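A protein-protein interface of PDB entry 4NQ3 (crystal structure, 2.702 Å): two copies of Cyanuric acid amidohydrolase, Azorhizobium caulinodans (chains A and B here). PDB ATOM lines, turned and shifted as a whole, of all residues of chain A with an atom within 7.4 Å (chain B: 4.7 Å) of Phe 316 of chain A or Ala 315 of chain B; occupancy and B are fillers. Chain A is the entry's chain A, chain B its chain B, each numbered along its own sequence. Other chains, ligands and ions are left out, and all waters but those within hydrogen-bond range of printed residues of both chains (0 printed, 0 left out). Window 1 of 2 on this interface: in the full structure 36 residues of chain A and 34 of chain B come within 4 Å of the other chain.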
ATOM      1  N   GLU A  83     -20.207  26.754  13.572  1.00  0.00           N
ATOM      2  CA  GLU A  83     -19.798  27.278  12.277  1.00  0.00           C
ATOM      3  C   GLU A  83     -20.668  28.455  11.899  1.00  0.00           C
ATOM      4  O   GLU A  83     -21.647  28.761  12.584  1.00  0.00           O
ATOM      5  CB  GLU A  83     -19.875  26.189  11.205  1.00  0.00           C
ATOM      6  CG  GLU A  83     -18.870  25.039  11.410  1.00  0.00           C
ATOM      7  CD  GLU A  83     -19.320  24.007  12.468  1.00  0.00           C
ATOM      8  OE1 GLU A  83     -20.439  24.147  13.023  1.00  0.00           O
ATOM      9  OE2 GLU A  83     -18.563  23.039  12.730  1.00  0.00           O
ATOM     10  N   GLY A  84     -20.320  29.119  10.803  1.00  0.00           N
ATOM     11  CA  GLY A  84     -21.084  30.276  10.405  1.00  0.00           C
ATOM     12  C   GLY A  84     -21.060  31.289  11.529  1.00  0.00           C
ATOM     13  O   GLY A  84     -20.018  31.531  12.138  1.00  0.00           O
ATOM     14  N   GLY A  85     -22.203  31.898  11.807  1.00  0.00           N
ATOM     15  CA  GLY A  85     -22.238  32.929  12.822  1.00  0.00           C
ATOM     16  C   GLY A  85     -22.702  32.395  14.158  1.00  0.00           C
ATOM     17  O   GLY A  85     -22.853  33.153  15.107  1.00  0.00           O
ATOM     18  N   MET A  86     -22.932  31.088  14.231  1.00  0.00           N
ATOM     19  CA  MET A  86     -23.499  30.479  15.432  1.00  0.00           C
ATOM     20  C   MET A  86     -22.658  30.831  16.646  1.00  0.00           C
ATOM     21  O   MET A  86     -21.439  30.748  16.588  1.00  0.00           O
ATOM     22  CB  MET A  86     -23.601  28.969  15.277  1.00  0.00           C
ATOM     23  CG  MET A  86     -24.400  28.318  16.373  1.00  0.00           C
ATOM     24  SD  MET A  86     -24.633  26.450  15.971  1.00  0.00           S
ATOM     25  CE  MET A  86     -23.787  26.444  14.195  1.00  0.00           C
ATOM     26  N   ASP A 258     -36.465  19.281   5.376  1.00  0.00           N
ATOM     27  CA  ASP A 258     -35.088  19.375   4.900  1.00  0.00           C
ATOM     28  C   ASP A 258     -34.370  20.591   5.519  1.00  0.00           C
ATOM     29  O   ASP A 258     -34.894  21.249   6.428  1.00  0.00           O
ATOM     30  CB  ASP A 258     -35.032  19.424   3.372  1.00  0.00           C
ATOM     31  CG  ASP A 258     -35.890  20.516   2.785  1.00  0.00           C
ATOM     32  OD1 ASP A 258     -36.041  21.571   3.441  1.00  0.00           O
ATOM     33  OD2 ASP A 258     -36.416  20.313   1.661  1.00  0.00           O
ATOM     34  N   ALA A 259     -33.172  20.872   5.010  1.00  0.00           N
ATOM     35  CA  ALA A 259     -32.262  21.828   5.628  1.00  0.00           C
ATOM     36  C   ALA A 259     -32.761  23.264   5.542  1.00  0.00           C
ATOM     37  O   ALA A 259     -32.263  24.131   6.251  1.00  0.00           O
ATOM     38  CB  ALA A 259     -30.878  21.711   5.018  1.00  0.00           C
ATOM     39  N   ILE A 260     -33.729  23.542   4.685  1.00  0.00           N
ATOM     40  CA  ILE A 260     -34.209  24.913   4.618  1.00  0.00           C
ATOM     41  C   ILE A 260     -35.690  25.013   4.958  1.00  0.00           C
ATOM     42  O   ILE A 260     -36.348  26.020   4.668  1.00  0.00           O
ATOM     43  CB  ILE A 260     -33.959  25.544   3.244  1.00  0.00           C
ATOM     44  CG1 ILE A 260     -34.606  24.707   2.147  1.00  0.00           C
ATOM     45  CG2 ILE A 260     -32.469  25.714   2.996  1.00  0.00           C
ATOM     46  CD1 ILE A 260     -34.384  25.266   0.794  1.00  0.00           C
ATOM     47  N   ALA A 286     -29.343  19.375  12.376  1.00  0.00           N
ATOM     48  CA  ALA A 286     -29.103  19.619  10.963  1.00  0.00           C
ATOM     49  C   ALA A 286     -28.387  18.425  10.372  1.00  0.00           C
ATOM     50  O   ALA A 286     -27.473  17.887  10.989  1.00  0.00           O
ATOM     51  CB  ALA A 286     -28.297  20.866  10.758  1.00  0.00           C
ATOM     52  N   ILE A 294     -30.860  18.847  -2.249  1.00  0.00           N
ATOM     53  CA  ILE A 294     -31.921  19.537  -1.527  1.00  0.00           C
ATOM     54  C   ILE A 294     -32.928  20.099  -2.541  1.00  0.00           C
ATOM     55  O   ILE A 294     -32.584  20.970  -3.361  1.00  0.00           O
ATOM     56  CB  ILE A 294     -31.373  20.668  -0.639  1.00  0.00           C
ATOM     57  CG1 ILE A 294     -30.307  20.110   0.310  1.00  0.00           C
ATOM     58  CG2 ILE A 294     -32.513  21.366   0.107  1.00  0.00           C
ATOM     59  CD1 ILE A 294     -29.673  21.137   1.210  1.00  0.00           C
ATOM     60  N   MET A 301     -21.997  18.576   0.283  1.00  0.00           N
ATOM     61  CA  MET A 301     -21.620  18.326   1.680  1.00  0.00           C
ATOM     62  C   MET A 301     -21.032  16.942   1.909  1.00  0.00           C
ATOM     63  O   MET A 301     -20.177  16.764   2.789  1.00  0.00           O
ATOM     64  CB  MET A 301     -22.818  18.523   2.599  1.00  0.00           C
ATOM     65  CG  MET A 301     -23.282  19.947   2.670  1.00  0.00           C
ATOM     66  SD  MET A 301     -24.748  20.176   3.905  1.00  0.00           S
ATOM     67  CE  MET A 301     -26.239  19.501   2.847  1.00  0.00           C
ATOM     68  N   THR A 310     -21.175  17.267   8.539  1.00  0.00           N
ATOM     69  CA  THR A 310     -21.940  17.910   9.607  1.00  0.00           C
ATOM     70  C   THR A 310     -21.516  19.341   9.869  1.00  0.00           C
ATOM     71  O   THR A 310     -22.329  20.174  10.285  1.00  0.00           O
ATOM     72  CB  THR A 310     -21.779  17.178  10.871  1.00  0.00           C
ATOM     73  OG1 THR A 310     -20.421  16.711  10.928  1.00  0.00           O
ATOM     74  CG2 THR A 310     -22.729  16.018  10.893  1.00  0.00           C
ATOM     75  N   ARG A 311     -20.233  19.615   9.646  1.00  0.00           N
ATOM     76  CA  ARG A 311     -19.715  20.969   9.742  1.00  0.00           C
ATOM     77  C   ARG A 311     -20.471  21.903   8.775  1.00  0.00           C
ATOM     78  O   ARG A 311     -20.903  23.004   9.174  1.00  0.00           O
ATOM     79  CB  ARG A 311     -18.217  20.963   9.450  1.00  0.00           C
ATOM     80  CG  ARG A 311     -17.392  21.862  10.318  1.00  0.00           C
ATOM     81  CD  ARG A 311     -16.300  21.079  11.003  1.00  0.00           C
ATOM     82  NE  ARG A 311     -15.092  21.887  11.239  1.00  0.00           N
ATOM     83  CZ  ARG A 311     -15.067  23.079  11.838  1.00  0.00           C
ATOM     84  NH1 ARG A 311     -16.185  23.660  12.259  1.00  0.00           N
ATOM     85  NH2 ARG A 311     -13.908  23.705  12.006  1.00  0.00           N
ATOM     86  N   HIS A 312     -20.667  21.445   7.528  1.00  0.00           N
ATOM     87  CA  HIS A 312     -21.493  22.167   6.554  1.00  0.00           C
ATOM     88  C   HIS A 312     -22.923  22.307   7.066  1.00  0.00           C
ATOM     89  O   HIS A 312     -23.412  23.414   7.257  1.00  0.00           O
ATOM     90  CB  HIS A 312     -21.528  21.450   5.192  1.00  0.00           C
ATOM     91  CG  HIS A 312     -20.283  21.616   4.373  1.00  0.00           C
ATOM     92  ND1 HIS A 312     -19.983  22.779   3.693  1.00  0.00           N
ATOM     93  CD2 HIS A 312     -19.274  20.753   4.103  1.00  0.00           C
ATOM     94  CE1 HIS A 312     -18.831  22.635   3.064  1.00  0.00           C
ATOM     95  NE2 HIS A 312     -18.381  21.414   3.294  1.00  0.00           N
ATOM     96  N   ALA A 313     -23.564  21.168   7.337  1.00  0.00           N
ATOM     97  CA  ALA A 313     -24.977  21.129   7.719  1.00  0.00           C
ATOM     98  C   ALA A 313     -25.274  22.111   8.838  1.00  0.00           C
ATOM     99  O   ALA A 313     -26.265  22.857   8.774  1.00  0.00           O
ATOM    100  CB  ALA A 313     -25.388  19.720   8.131  1.00  0.00           C
ATOM    101  N   ARG A 314     -24.405  22.126   9.850  1.00  0.00           N
ATOM    102  CA  ARG A 314     -24.591  23.019  10.986  1.00  0.00           C
ATOM    103  C   ARG A 314     -24.579  24.481  10.555  1.00  0.00           C
ATOM    104  O   ARG A 314     -25.540  25.207  10.812  1.00  0.00           O
ATOM    105  CB  ARG A 314     -23.523  22.791  12.055  1.00  0.00           C
ATOM    106  CG  ARG A 314     -23.802  21.676  13.054  1.00  0.00           C
ATOM    107  CD  ARG A 314     -22.816  21.765  14.235  1.00  0.00           C
ATOM    108  NE  ARG A 314     -21.438  21.626  13.790  1.00  0.00           N
ATOM    109  CZ  ARG A 314     -20.785  20.472  13.771  1.00  0.00           C
ATOM    110  NH1 ARG A 314     -21.387  19.368  14.220  1.00  0.00           N
ATOM    111  NH2 ARG A 314     -19.534  20.426  13.327  1.00  0.00           N
ATOM    112  N   ALA A 315     -23.494  24.912   9.914  1.00  0.00           N
ATOM    113  CA  ALA A 315     -23.404  26.290   9.417  1.00  0.00           C
ATOM    114  C   ALA A 315     -24.643  26.665   8.598  1.00  0.00           C
ATOM    115  O   ALA A 315     -25.212  27.737   8.777  1.00  0.00           O
ATOM    116  CB  ALA A 315     -22.141  26.486   8.585  1.00  0.00           C
ATOM    117  N   PHE A 316     -25.066  25.771   7.713  1.00  0.00           N
ATOM    118  CA  PHE A 316     -26.166  26.066   6.810  1.00  0.00           C
ATOM    119  C   PHE A 316     -27.487  26.193   7.544  1.00  0.00           C
ATOM    120  O   PHE A 316     -28.169  27.214   7.434  1.00  0.00           O
ATOM    121  CB  PHE A 316     -26.282  24.987   5.746  1.00  0.00           C
ATOM    122  CG  PHE A 316     -27.112  25.389   4.578  1.00  0.00           C
ATOM    123  CD1 PHE A 316     -26.691  26.422   3.730  1.00  0.00           C
ATOM    124  CD2 PHE A 316     -28.318  24.731   4.305  1.00  0.00           C
ATOM    125  CE1 PHE A 316     -27.461  26.797   2.632  1.00  0.00           C
ATOM    126  CE2 PHE A 316     -29.107  25.100   3.193  1.00  0.00           C
ATOM    127  CZ  PHE A 316     -28.676  26.131   2.361  1.00  0.00           C
ATOM    128  N   VAL A 317     -27.843  25.178   8.321  1.00  0.00           N
ATOM    129  CA  VAL A 317     -29.103  25.246   9.047  1.00  0.00           C
ATOM    130  C   VAL A 317     -29.085  26.352  10.118  1.00  0.00           C
ATOM    131  O   VAL A 317     -30.119  26.961  10.382  1.00  0.00           O
ATOM    132  CB  VAL A 317     -29.439  23.897   9.721  1.00  0.00           C
ATOM    133  CG1 VAL A 317     -30.642  24.039  10.668  1.00  0.00           C
ATOM    134  CG2 VAL A 317     -29.662  22.817   8.670  1.00  0.00           C
ATOM    135  N   ALA A 318     -27.931  26.628  10.728  1.00  0.00           N
ATOM    136  CA  ALA A 318     -27.875  27.688  11.739  1.00  0.00           C
ATOM    137  C   ALA A 318     -28.275  29.016  11.100  1.00  0.00           C
ATOM    138  O   ALA A 318     -29.038  29.800  11.673  1.00  0.00           O
ATOM    139  CB  ALA A 318     -26.490  27.783  12.379  1.00  0.00           C
ATOM    140  N   GLY A 319     -27.783  29.237   9.886  1.00  0.00           N
ATOM    141  CA  GLY A 319     -28.123  30.429   9.144  1.00  0.00           C
ATOM    142  C   GLY A 319     -29.613  30.511   8.856  1.00  0.00           C
ATOM    143  O   GLY A 319     -30.225  31.552   9.083  1.00  0.00           O
ATOM    144  N   ALA A 320     -30.215  29.425   8.372  1.00  0.00           N
ATOM    145  CA  ALA A 320     -31.649  29.451   8.095  1.00  0.00           C
ATOM    146  C   ALA A 320     -32.457  29.831   9.360  1.00  0.00           C
ATOM    147  O   ALA A 320     -33.222  30.795   9.342  1.00  0.00           O
ATOM    148  CB  ALA A 320     -32.111  28.100   7.544  1.00  0.00           C
ATOM    149  N   LEU A 321     -32.241  29.122  10.469  1.00  0.00           N
ATOM    150  CA  LEU A 321     -32.974  29.382  11.715  1.00  0.00           C
ATOM    151  C   LEU A 321     -32.702  30.786  12.293  1.00  0.00           C
ATOM    152  O   LEU A 321     -33.614  31.472  12.767  1.00  0.00           O
ATOM    153  CB  LEU A 321     -32.629  28.315  12.751  1.00  0.00           C
ATOM    154  CG  LEU A 321     -33.097  26.910  12.394  1.00  0.00           C
ATOM    155  CD1 LEU A 321     -32.694  25.915  13.445  1.00  0.00           C
ATOM    156  CD2 LEU A 321     -34.578  26.882  12.217  1.00  0.00           C
ATOM    157  N   ALA A 322     -31.434  31.189  12.277  1.00  0.00           N
ATOM    158  CA  ALA A 322     -31.038  32.505  12.756  1.00  0.00           C
ATOM    159  C   ALA A 322     -31.733  33.602  11.965  1.00  0.00           C
ATOM    160  O   ALA A 322     -32.102  34.642  12.510  1.00  0.00           O
ATOM    161  CB  ALA A 322     -29.533  32.666  12.662  1.00  0.00           C
ATOM    162  N   VAL A 332     -27.565  24.279  17.527  1.00  0.00           N
ATOM    163  CA  VAL A 332     -27.695  23.459  16.324  1.00  0.00           C
ATOM    164  C   VAL A 332     -26.654  22.360  16.309  1.00  0.00           C
ATOM    165  O   VAL A 332     -25.474  22.615  16.448  1.00  0.00           O
ATOM    166  CB  VAL A 332     -27.522  24.283  15.057  1.00  0.00           C
ATOM    167  CG1 VAL A 332     -27.670  23.399  13.832  1.00  0.00           C
ATOM    168  CG2 VAL A 332     -28.519  25.416  15.043  1.00  0.00           C
ATOM    169  N   GLU B  83     -20.401  26.182   0.107  1.00  0.00           N
ATOM    170  CA  GLU B  83     -20.517  25.558   1.416  1.00  0.00           C
ATOM    171  C   GLU B  83     -21.977  25.352   1.757  1.00  0.00           C
ATOM    172  O   GLU B  83     -22.839  25.770   0.993  1.00  0.00           O
ATOM    173  CB  GLU B  83     -19.832  26.417   2.469  1.00  0.00           C
ATOM    174  CG  GLU B  83     -18.333  26.499   2.255  1.00  0.00           C
ATOM    175  CD  GLU B  83     -17.925  27.532   1.211  1.00  0.00           C
ATOM    176  OE1 GLU B  83     -18.798  28.274   0.713  1.00  0.00           O
ATOM    177  OE2 GLU B  83     -16.725  27.589   0.868  1.00  0.00           O
ATOM    178  N   GLY B  84     -22.256  24.678   2.869  1.00  0.00           N
ATOM    179  CA  GLY B  84     -23.630  24.419   3.256  1.00  0.00           C
ATOM    180  C   GLY B  84     -24.369  23.691   2.147  1.00  0.00           C
ATOM    181  O   GLY B  84     -23.821  22.804   1.504  1.00  0.00           O
ATOM    182  N   GLY B  85     -25.612  24.087   1.899  1.00  0.00           N
ATOM    183  CA  GLY B  85     -26.428  23.419   0.906  1.00  0.00           C
ATOM    184  C   GLY B  85     -26.388  24.137  -0.423  1.00  0.00           C
ATOM    185  O   GLY B  85     -27.112  23.787  -1.359  1.00  0.00           O
ATOM    186  N   MET B  86     -25.537  25.152  -0.505  1.00  0.00           N
ATOM    187  CA  MET B  86     -25.484  25.990  -1.687  1.00  0.00           C
ATOM    188  C   MET B  86     -25.169  25.103  -2.868  1.00  0.00           C
ATOM    189  O   MET B  86     -24.231  24.316  -2.813  1.00  0.00           O
ATOM    190  CB  MET B  86     -24.443  27.087  -1.527  1.00  0.00           C
ATOM    191  CG  MET B  86     -24.807  28.373  -2.232  1.00  0.00           C
ATOM    192  SD  MET B  86     -23.309  29.621  -2.297  1.00  0.00           S
ATOM    193  CE  MET B  86     -22.614  29.376  -0.491  1.00  0.00           C
ATOM    194  N   ARG B 311     -15.426  31.181   3.939  1.00  0.00           N
ATOM    195  CA  ARG B 311     -16.127  29.893   3.848  1.00  0.00           C
ATOM    196  C   ARG B 311     -17.283  29.831   4.871  1.00  0.00           C
ATOM    197  O   ARG B 311     -18.375  29.364   4.551  1.00  0.00           O
ATOM    198  CB  ARG B 311     -15.167  28.715   4.058  1.00  0.00           C
ATOM    199  CG  ARG B 311     -14.257  28.365   2.900  1.00  0.00           C
ATOM    200  CD  ARG B 311     -13.172  27.380   3.346  1.00  0.00           C
ATOM    201  NE  ARG B 311     -13.178  26.010   2.772  1.00  0.00           N
ATOM    202  CZ  ARG B 311     -14.102  25.463   1.970  1.00  0.00           C
ATOM    203  NH1 ARG B 311     -15.186  26.125   1.590  1.00  0.00           N
ATOM    204  NH2 ARG B 311     -13.939  24.213   1.542  1.00  0.00           N
ATOM    205  N   HIS B 312     -17.034  30.286   6.099  1.00  0.00           N
ATOM    206  CA  HIS B 312     -18.095  30.412   7.109  1.00  0.00           C
ATOM    207  C   HIS B 312     -19.217  31.343   6.653  1.00  0.00           C
ATOM    208  O   HIS B 312     -20.392  30.969   6.672  1.00  0.00           O
ATOM    209  CB  HIS B 312     -17.552  30.947   8.439  1.00  0.00           C
ATOM    210  CG  HIS B 312     -16.873  29.925   9.288  1.00  0.00           C
ATOM    211  ND1 HIS B 312     -17.570  28.991  10.024  1.00  0.00           N
ATOM    212  CD2 HIS B 312     -15.562  29.717   9.555  1.00  0.00           C
ATOM    213  CE1 HIS B 312     -16.714  28.239  10.696  1.00  0.00           C
ATOM    214  NE2 HIS B 312     -15.490  28.660  10.430  1.00  0.00           N
ATOM    215  N   ALA B 313     -18.862  32.575   6.309  1.00  0.00           N
ATOM    216  CA  ALA B 313     -19.858  33.571   5.935  1.00  0.00           C
ATOM    217  C   ALA B 313     -20.809  33.064   4.823  1.00  0.00           C
ATOM    218  O   ALA B 313     -22.030  33.220   4.907  1.00  0.00           O
ATOM    219  CB  ALA B 313     -19.156  34.871   5.501  1.00  0.00           C
ATOM    220  N   ARG B 314     -20.243  32.448   3.791  1.00  0.00           N
ATOM    221  CA  ARG B 314     -21.029  31.961   2.668  1.00  0.00           C
ATOM    222  C   ARG B 314     -22.028  30.926   3.152  1.00  0.00           C
ATOM    223  O   ARG B 314     -23.232  31.053   2.933  1.00  0.00           O
ATOM    224  CB  ARG B 314     -20.125  31.361   1.589  1.00  0.00           C
ATOM    225  CG  ARG B 314     -19.487  32.363   0.689  1.00  0.00           C
ATOM    226  CD  ARG B 314     -18.812  31.690  -0.478  1.00  0.00           C
ATOM    227  NE  ARG B 314     -17.751  30.764  -0.086  1.00  0.00           N
ATOM    228  CZ  ARG B 314     -16.465  31.104   0.025  1.00  0.00           C
ATOM    229  NH1 ARG B 314     -16.082  32.352  -0.192  1.00  0.00           N
ATOM    230  NH2 ARG B 314     -15.552  30.203   0.365  1.00  0.00           N
ATOM    231  N   ALA B 315     -21.512  29.894   3.810  1.00  0.00           N
ATOM    232  CA  ALA B 315     -22.359  28.855   4.360  1.00  0.00           C
ATOM    233  C   ALA B 315     -23.496  29.471   5.147  1.00  0.00           C
ATOM    234  O   ALA B 315     -24.638  29.149   4.917  1.00  0.00           O
ATOM    235  CB  ALA B 315     -21.554  27.929   5.246  1.00  0.00           C
ATOM    236  N   PHE B 316     -23.185  30.419   6.017  1.00  0.00           N
ATOM    237  CA  PHE B 316     -24.178  30.974   6.926  1.00  0.00           C
ATOM    238  C   PHE B 316     -25.234  31.819   6.222  1.00  0.00           C
ATOM    239  O   PHE B 316     -26.419  31.579   6.429  1.00  0.00           O
ATOM    240  CB  PHE B 316     -23.485  31.794   8.018  1.00  0.00           C
ATOM    241  CG  PHE B 316     -24.337  32.051   9.226  1.00  0.00           C
ATOM    242  CD1 PHE B 316     -24.744  31.009  10.037  1.00  0.00           C
ATOM    243  CD2 PHE B 316     -24.694  33.339   9.583  1.00  0.00           C
ATOM    244  CE1 PHE B 316     -25.520  31.241  11.170  1.00  0.00           C
ATOM    245  CE2 PHE B 316     -25.467  33.582  10.723  1.00  0.00           C
ATOM    246  CZ  PHE B 316     -25.883  32.529  11.508  1.00  0.00           C
ATOM    247  N   VAL B 317     -24.845  32.821   5.424  1.00  0.00           N
ATOM    248  CA  VAL B 317     -25.882  33.619   4.748  1.00  0.00           C
ATOM    249  C   VAL B 317     -26.590  32.818   3.647  1.00  0.00           C
ATOM    250  O   VAL B 317     -27.773  33.038   3.405  1.00  0.00           O
ATOM    251  CB  VAL B 317     -25.372  34.968   4.139  1.00  0.00           C
ATOM    252  CG1 VAL B 317     -24.164  35.496   4.879  1.00  0.00           C
ATOM    253  CG2 VAL B 317     -25.127  34.830   2.659  1.00  0.00           C
ATOM    254  N   ALA B 318     -25.900  31.884   2.994  1.00  0.00           N
ATOM    255  CA  ALA B 318     -26.569  31.068   1.980  1.00  0.00           C
ATOM    256  C   ALA B 318     -27.737  30.347   2.625  1.00  0.00           C
ATOM    257  O   ALA B 318     -28.807  30.247   2.049  1.00  0.00           O
ATOM    258  CB  ALA B 318     -25.619  30.075   1.344  1.00  0.00           C
ATOM    259  N   GLY B 319     -27.525  29.844   3.828  1.00  0.00           N
ATOM    260  CA  GLY B 319     -28.584  29.221   4.584  1.00  0.00           C
ATOM    261  C   GLY B 319     -29.677  30.207   4.935  1.00  0.00           C
ATOM    262  O   GLY B 319     -30.856  29.898   4.796  1.00  0.00           O
ATOM    263  N   ALA B 322     -31.575  31.035   1.605  1.00  0.00           N
ATOM    264  CA  ALA B 322     -32.331  29.887   1.111  1.00  0.00           C
ATOM    265  C   ALA B 322     -33.593  29.626   1.942  1.00  0.00           C
ATOM    266  O   ALA B 322     -34.604  29.150   1.422  1.00  0.00           O
ATOM    267  CB  ALA B 322     -31.456  28.646   1.066  1.00  0.00           C
ATOM    268  N   THR B 328     -31.883  26.334  -3.172  1.00  0.00           N
ATOM    269  CA  THR B 328     -30.471  26.510  -2.821  1.00  0.00           C
ATOM    270  C   THR B 328     -29.570  26.939  -3.961  1.00  0.00           C
ATOM    271  O   THR B 328     -28.351  26.991  -3.808  1.00  0.00           O
ATOM    272  CB  THR B 328     -29.882  25.225  -2.262  1.00  0.00           C
ATOM    273  OG1 THR B 328     -30.011  24.197  -3.246  1.00  0.00           O
ATOM    274  CG2 THR B 328     -30.600  24.814  -0.974  1.00  0.00           C
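Printed residues of chain A that touch a printed residue of chain B: Glu 83, Gly 84, Gly 85, Ile 260, Ile 294, Met 301, His 312, Ala 315, Phe 316, Ala 318, Gly 319, Ala 320 and Ala 322. Of the 15 printed residues of chain B, 9 touch a printed residue of chain A. Printed residues of chain B that touch a printed residue of chain A: Glu 83, Gly 84, Gly 85, His 312, Ala 315, Phe 316, Ala 318, Gly 319 and Ala 322. Hydrophobic or aromatic side chains of chain B within 4 Å of the printed part of chain A: His 312, Ala 315, Phe 316, Ala 318 and Ala 322. Among the printed residues, 22 pairs touch across the chains. Among the printed residues, no Asp or Glu carboxylate lies within 4 Å of a Lys or Arg side-chain nitrogen of the other chain.
Among the printed residues, merely in contact across the chains: Phe 316 of chain A with Gly 85 of chain B, Gly 85 of chain A with Phe 316 of chain B, Phe 316 of chain A with Gly 319 of chain B, Gly 319 of chain A with Phe 316 of chain B, Ala 320 of chain A with Gly 319 of chain B, Ala 315 of chain A with Phe 316 of chain B, Ala 318 of chain A with Phe 316 of chain B, Phe 316 of chain A with Ala 318 of chain B, Glu 83 of chain A with His 312 of chain B, Phe 316 of chain A with Ala 315 of chain B, His 312 of chain A with Glu 83 of chain B, Ile 260 of chain A with Ala 322 of chain B, Phe 316 of chain A with Gly 84 of chain B, Ala 315 of chain A with Ala 315 of chain B, Gly 84 of chain A with Phe 316 of chain B, Ala 322 of chain A with Phe 316 of chain B, Gly 319 of chain A with Gly 319 of chain B, Phe 316 of chain A with Ala 322 of chain B and Ile 294 of chain A with Gly 85 of chain B.
Gly 84 of chain A touches Phe 316 of chain B, and with the chains exchanged Phe 316 of chain A touches Gly 84 of chain B. Gly 85 of chain A touches Phe 316 of chain B, and with the chains exchanged Phe 316 of chain A touches Gly 85 of chain B. Phe 316 of chain A touches Ala 322 of chain B, and with the chains exchanged Ala 322 of chain A touches Phe 316 of chain B. Gly 319 of chain A touches its own counterpart, Gly 319 of chain B. Of the 22 pairs that touch across the chains among the printed residues, 18 have their exchanged pair printed and touching as well.
ND1 of His 312 of chain A is in hydrogen-bond range of N of Gly 84 of chain B (3.1 Å). N of Gly 84 of chain A is in hydrogen-bond range of ND1 of His 312 of chain B, at 2.9 Å. The side-chain sulfur (SD) of Met 301 of chain A lies close to the backbone carbonyl oxygen (O) of Gly 84 of chain B (3.7 Å).
OE1 of Glu 83 of chain B lies within salt-bridge range of NE of Arg 314 of chain B. OE2 of Glu 83 of chain A lies within salt-bridge range of NH1 of Arg 311 of chain A (2.5 Å). OD1 of Asp 258 of chain A sits close to N of Ile 260 of chain A. The side-chain sulfur (SD) of Met 301 of chain A lies within hydrogen-bond range of the backbone NH (N) of Ala 313 of chain A (3.8 Å). The backbone carbonyl oxygen of Gly 85 of chain B sits close to the side-chain hydroxyl of Thr 328 of chain B, at 3.5 Å. The guanidinium group (NE) of Arg 314 of chain A lies within salt-bridge range of the side-chain carboxylate (OE1) of Glu 83 of chain A, at 2.8 Å.
Phe 316 of chain A touches six residues of chain B. Ala 315 of chain B touches just these residues of chain A: Ala 315 (3.7 Å) and Phe 316 (3.6 Å). Printed residues of chain B within 4 Å of Glu 83 of chain A: His 312. Printed residues of chain A within 4 Å of Gly 85 of chain B: Ile 294 and Phe 316. Arg 314 of chain B touches none of the printed residues of chain A. Met 86 of chain A touches none of the printed residues of chain B. The nearest residue of chain B that does not touch Phe 316 of chain A is Met 86 of chain B (4.03 Å). The nearest printed residue of chain B that does not touch Glu 83 of chain A is Phe 316 of chain B (4.6 Å).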
